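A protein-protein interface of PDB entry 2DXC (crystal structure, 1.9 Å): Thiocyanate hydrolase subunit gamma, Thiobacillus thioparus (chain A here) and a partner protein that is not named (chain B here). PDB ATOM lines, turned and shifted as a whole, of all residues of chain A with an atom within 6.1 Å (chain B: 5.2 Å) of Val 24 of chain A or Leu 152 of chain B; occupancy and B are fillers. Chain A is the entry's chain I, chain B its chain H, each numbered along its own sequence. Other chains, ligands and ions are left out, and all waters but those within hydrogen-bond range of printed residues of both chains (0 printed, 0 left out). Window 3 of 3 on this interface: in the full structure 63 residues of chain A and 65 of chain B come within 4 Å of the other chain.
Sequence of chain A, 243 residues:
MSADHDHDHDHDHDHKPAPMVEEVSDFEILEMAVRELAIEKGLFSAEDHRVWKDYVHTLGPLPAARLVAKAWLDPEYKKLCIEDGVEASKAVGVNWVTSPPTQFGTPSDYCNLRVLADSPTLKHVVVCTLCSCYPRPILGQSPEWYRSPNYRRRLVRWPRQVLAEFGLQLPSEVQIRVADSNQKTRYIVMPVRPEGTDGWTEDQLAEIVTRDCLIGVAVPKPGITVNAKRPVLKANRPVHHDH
NH1 of Arg 237 of chain A sits close to O of Tyr 151 of chain B (3.4 Å).
The backbone carbonyl oxygen (O) of Glu 23 of chain A is in hydrogen-bond range of the guanidinium group (NH2) of Arg 237 of chain A (3.2 Å).
The backbone NH (N) of Ser 25 of chain A is in hydrogen-bond range of the side-chain carboxylate (OE1) of Glu 28 of chain A (3.0 Å).
OE2 of Glu 28 of chain A lies within salt-bridge range of NE of Arg 237 of chain A, 2.7 Å away.
CG1 of Val 142 of chain B touches CG2 of Val 24 of chain A, 3.98 Å away.
CD2 of Leu 148 of chain B touches CG1 of Val 24 of chain A, at 3.5 Å.
Leu 152 of chain B touches Val 24 of chain A.
Tyr 151 of chain B touches Glu 28 of chain A (CD1 to OE2, 3.6 Å).
Glu 23 of chain A touches none of the printed residues of chain B.
Printed residues of chain B within 4 Å of Val 24 of chain A: Val 142, Leu 148 and Leu 152.
Printed residues of chain A within 4 Å of Leu 148 of chain B: Val 24.
Gly 149 of chain B touches none of the printed residues of chain A.
Printed residues of chain A within 4 Å of Tyr 151 of chain B: Glu 28 (3.6 Å) and Arg 237 (3.4 Å).
Printed residues of chain A within 4 Å of Leu 152 of chain B: Val 24 (3.997 Å).
The nearest printed residue of chain B that does not touch Val 24 of chain A is Tyr 151 of chain B (4.7 Å).
The nearest printed residue of chain A that does not touch Leu 152 of chain B is Glu 23 of chain A (4.7 Å).
The nearest printed residue of chain A that does not touch Tyr 151 of chain B is Val 24 of chain A (4.7 Å).
Along chain A the printed residues that touch a printed residue of chain B span positions 24 to 237.
Of the 9 printed residues of chain B, 4 touch a printed residue of chain A.
Along chain B the printed residues that touch a printed residue of chain A span positions 142 to 152.
Among the printed residues, 5 pairs touch across the chains.
Among the printed residues, no Asp or Glu carboxylate lies within 4 Å of a Lys or Arg side-chain nitrogen of the other chain.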
ATOM      1  N   GLU A  23      14.997  18.985  19.615  1.00  0.00           N
ATOM      2  CA  GLU A  23      14.574  18.174  20.795  1.00  0.00           C
ATOM      3  C   GLU A  23      14.951  16.709  20.574  1.00  0.00           C
ATOM      4  O   GLU A  23      14.386  15.806  21.197  1.00  0.00           O
ATOM      5  CB  GLU A  23      13.058  18.286  20.994  1.00  0.00           C
ATOM      6  CG  GLU A  23      12.556  17.655  22.285  1.00  0.00           C
ATOM      7  CD  GLU A  23      11.067  17.358  22.253  1.00  0.00           C
ATOM      8  OE1 GLU A  23      10.517  16.964  23.306  1.00  0.00           O
ATOM      9  OE2 GLU A  23      10.448  17.510  21.176  1.00  0.00           O
ATOM     10  N   VAL A  24      15.911  16.482  19.684  1.00  0.00           N
ATOM     11  CA  VAL A  24      16.370  15.135  19.363  1.00  0.00           C
ATOM     12  C   VAL A  24      17.084  14.483  20.550  1.00  0.00           C
ATOM     13  O   VAL A  24      17.945  15.094  21.180  1.00  0.00           O
ATOM     14  CB  VAL A  24      17.316  15.178  18.149  1.00  0.00           C
ATOM     15  CG1 VAL A  24      17.815  13.785  17.815  1.00  0.00           C
ATOM     16  CG2 VAL A  24      16.587  15.788  16.959  1.00  0.00           C
ATOM     17  N   SER A  25      16.722  13.240  20.850  1.00  0.00           N
ATOM     18  CA  SER A  25      17.327  12.516  21.964  1.00  0.00           C
ATOM     19  C   SER A  25      18.560  11.736  21.522  1.00  0.00           C
ATOM     20  O   SER A  25      18.809  11.563  20.327  1.00  0.00           O
ATOM     21  CB  SER A  25      16.323  11.533  22.562  1.00  0.00           C
ATOM     22  OG  SER A  25      16.109  10.444  21.684  1.00  0.00           O
ATOM     23  N   ASP A  26      19.326  11.256  22.495  1.00  0.00           N
ATOM     24  CA  ASP A  26      20.518  10.471  22.199  1.00  0.00           C
ATOM     25  C   ASP A  26      20.135   9.186  21.460  1.00  0.00           C
ATOM     26  O   ASP A  26      20.911   8.672  20.660  1.00  0.00           O
ATOM     27  CB  ASP A  26      21.265  10.135  23.496  1.00  0.00           C
ATOM     28  CG  ASP A  26      21.982  11.339  24.089  1.00  0.00           C
ATOM     29  OD1 ASP A  26      22.871  11.900  23.411  1.00  0.00           O
ATOM     30  OD2 ASP A  26      21.662  11.728  25.230  1.00  0.00           O
ATOM     31  N   GLU A  28      17.588   8.829  19.267  1.00  0.00           N
ATOM     32  CA  GLU A  28      17.284   9.149  17.878  1.00  0.00           C
ATOM     33  C   GLU A  28      18.570   9.387  17.089  1.00  0.00           C
ATOM     34  O   GLU A  28      18.674   8.996  15.925  1.00  0.00           O
ATOM     35  CB  GLU A  28      16.342  10.362  17.822  1.00  0.00           C
ATOM     36  CG  GLU A  28      15.008  10.063  18.517  1.00  0.00           C
ATOM     37  CD  GLU A  28      14.095  11.269  18.660  1.00  0.00           C
ATOM     38  OE1 GLU A  28      14.600  12.385  18.884  1.00  0.00           O
ATOM     39  OE2 GLU A  28      12.862  11.092  18.571  1.00  0.00           O
ATOM     40  N   ILE A  29      19.557  10.008  17.723  1.00  0.00           N
ATOM     41  CA  ILE A  29      20.837  10.249  17.067  1.00  0.00           C
ATOM     42  C   ILE A  29      21.516   8.908  16.785  1.00  0.00           C
ATOM     43  O   ILE A  29      22.019   8.666  15.684  1.00  0.00           O
ATOM     44  CB  ILE A  29      21.775  11.094  17.955  1.00  0.00           C
ATOM     45  CG1 ILE A  29      21.273  12.539  18.007  1.00  0.00           C
ATOM     46  CG2 ILE A  29      23.211  11.039  17.412  1.00  0.00           C
ATOM     47  CD1 ILE A  29      21.939  13.384  19.072  1.00  0.00           C
ATOM     48  N   ASN A 236       7.697  10.580  23.193  1.00  0.00           N
ATOM     49  CA  ASN A 236       8.163  11.933  22.938  1.00  0.00           C
ATOM     50  C   ASN A 236       7.868  12.265  21.478  1.00  0.00           C
ATOM     51  O   ASN A 236       7.495  13.388  21.148  1.00  0.00           O
ATOM     52  CB  ASN A 236       9.664  12.029  23.218  1.00  0.00           C
ATOM     53  CG  ASN A 236      10.212  13.423  22.990  1.00  0.00           C
ATOM     54  OD1 ASN A 236       9.778  14.383  23.626  1.00  0.00           O
ATOM     55  ND2 ASN A 236      11.175  13.542  22.080  1.00  0.00           N
ATOM     56  N   ARG A 237       8.020  11.268  20.610  1.00  0.00           N
ATOM     57  CA  ARG A 237       7.776  11.438  19.179  1.00  0.00           C
ATOM     58  C   ARG A 237       7.169  10.137  18.641  1.00  0.00           C
ATOM     59  O   ARG A 237       7.859   9.332  18.015  1.00  0.00           O
ATOM     60  CB  ARG A 237       9.098  11.739  18.472  1.00  0.00           C
ATOM     61  CG  ARG A 237       8.975  12.609  17.236  1.00  0.00           C
ATOM     62  CD  ARG A 237      10.322  12.738  16.536  1.00  0.00           C
ATOM     63  NE  ARG A 237      11.402  13.070  17.463  1.00  0.00           N
ATOM     64  CZ  ARG A 237      11.553  14.245  18.068  1.00  0.00           C
ATOM     65  NH1 ARG A 237      10.690  15.228  17.848  1.00  0.00           N
ATOM     66  NH2 ARG A 237      12.567  14.435  18.900  1.00  0.00           N
ATOM     67  N   VAL B 142      22.005  17.954  13.503  1.00  0.00           N
ATOM     68  CA  VAL B 142      20.919  18.496  14.316  1.00  0.00           C
ATOM     69  C   VAL B 142      21.209  19.922  14.774  1.00  0.00           C
ATOM     70  O   VAL B 142      20.355  20.805  14.670  1.00  0.00           O
ATOM     71  CB  VAL B 142      20.675  17.636  15.575  1.00  0.00           C
ATOM     72  CG1 VAL B 142      19.636  18.305  16.475  1.00  0.00           C
ATOM     73  CG2 VAL B 142      20.214  16.250  15.173  1.00  0.00           C
ATOM     74  N   GLY B 147      18.265  19.504  10.040  1.00  0.00           N
ATOM     75  CA  GLY B 147      17.168  18.591  10.298  1.00  0.00           C
ATOM     76  C   GLY B 147      17.722  17.187  10.461  1.00  0.00           C
ATOM     77  O   GLY B 147      18.875  16.928  10.111  1.00  0.00           O
ATOM     78  N   LEU B 148      16.913  16.279  10.996  1.00  0.00           N
ATOM     79  CA  LEU B 148      17.349  14.904  11.192  1.00  0.00           C
ATOM     80  C   LEU B 148      16.269  13.931  10.730  1.00  0.00           C
ATOM     81  O   LEU B 148      15.449  13.468  11.526  1.00  0.00           O
ATOM     82  CB  LEU B 148      17.678  14.657  12.666  1.00  0.00           C
ATOM     83  CG  LEU B 148      18.297  13.293  12.983  1.00  0.00           C
ATOM     84  CD1 LEU B 148      19.611  13.155  12.237  1.00  0.00           C
ATOM     85  CD2 LEU B 148      18.522  13.150  14.481  1.00  0.00           C
ATOM     86  N   GLY B 149      16.271  13.633   9.435  1.00  0.00           N
ATOM     87  CA  GLY B 149      15.290  12.717   8.881  1.00  0.00           C
ATOM     88  C   GLY B 149      13.876  12.990   9.353  1.00  0.00           C
ATOM     89  O   GLY B 149      13.412  14.128   9.328  1.00  0.00           O
ATOM     90  N   GLU B 150      13.193  11.941   9.795  1.00  0.00           N
ATOM     91  CA  GLU B 150      11.823  12.067  10.268  1.00  0.00           C
ATOM     92  C   GLU B 150      11.740  12.529  11.721  1.00  0.00           C
ATOM     93  O   GLU B 150      10.647  12.724  12.250  1.00  0.00           O
ATOM     94  CB  GLU B 150      11.096  10.726  10.091  1.00  0.00           C
ATOM     95  CG  GLU B 150      11.762   9.556  10.800  1.00  0.00           C
ATOM     96  CD  GLU B 150      11.308   8.207  10.262  1.00  0.00           C
ATOM     97  OE1 GLU B 150      10.080   7.999  10.124  1.00  0.00           O
ATOM     98  OE2 GLU B 150      12.184   7.354   9.985  1.00  0.00           O
ATOM     99  N   TYR B 151      12.891  12.718  12.360  1.00  0.00           N
ATOM    100  CA  TYR B 151      12.928  13.153  13.755  1.00  0.00           C
ATOM    101  C   TYR B 151      12.877  14.670  13.928  1.00  0.00           C
ATOM    102  O   TYR B 151      12.391  15.170  14.943  1.00  0.00           O
ATOM    103  CB  TYR B 151      14.188  12.618  14.441  1.00  0.00           C
ATOM    104  CG  TYR B 151      14.287  11.109  14.450  1.00  0.00           C
ATOM    105  CD1 TYR B 151      13.296  10.330  15.050  1.00  0.00           C
ATOM    106  CD2 TYR B 151      15.358  10.459  13.846  1.00  0.00           C
ATOM    107  CE1 TYR B 151      13.373   8.939  15.046  1.00  0.00           C
ATOM    108  CE2 TYR B 151      15.447   9.068  13.836  1.00  0.00           C
ATOM    109  CZ  TYR B 151      14.450   8.316  14.437  1.00  0.00           C
ATOM    110  OH  TYR B 151      14.528   6.943  14.419  1.00  0.00           O
ATOM    111  N   LEU B 152      13.385  15.402  12.944  1.00  0.00           N
ATOM    112  CA  LEU B 152      13.402  16.855  13.024  1.00  0.00           C
ATOM    113  C   LEU B 152      13.468  17.464  11.633  1.00  0.00           C
ATOM    114  O   LEU B 152      14.363  17.149  10.852  1.00  0.00           O
ATOM    115  CB  LEU B 152      14.617  17.314  13.834  1.00  0.00           C
ATOM    116  CG  LEU B 152      14.758  18.816  14.087  1.00  0.00           C
ATOM    117  CD1 LEU B 152      13.703  19.260  15.090  1.00  0.00           C
ATOM    118  CD2 LEU B 152      16.152  19.120  14.621  1.00  0.00           C
ATOM    119  N   PRO B 153      12.514  18.346  11.301  1.00  0.00           N
ATOM    120  CA  PRO B 153      12.514  18.976   9.979  1.00  0.00           C
ATOM    121  C   PRO B 153      13.598  20.051   9.873  1.00  0.00           C
ATOM    122  O   PRO B 153      14.053  20.587  10.885  1.00  0.00           O
ATOM    123  CB  PRO B 153      11.106  19.557   9.880  1.00  0.00           C
ATOM    124  CG  PRO B 153      10.828  19.959  11.295  1.00  0.00           C
ATOM    125  CD  PRO B 153      11.338  18.764  12.087  1.00  0.00           C
ATOM    126  N   PRO B 154      14.035  20.362   8.645  1.00  0.00           N
ATOM    127  CA  PRO B 154      15.068  21.381   8.445  1.00  0.00           C
ATOM    128  C   PRO B 154      14.551  22.750   8.867  1.00  0.00           C
ATOM    129  O   PRO B 154      13.370  22.913   9.167  1.00  0.00           O
ATOM    130  CB  PRO B 154      15.330  21.318   6.941  1.00  0.00           C
ATOM    131  CG  PRO B 154      14.999  19.902   6.594  1.00  0.00           C
ATOM    132  CD  PRO B 154      13.734  19.672   7.379  1.00  0.00           C
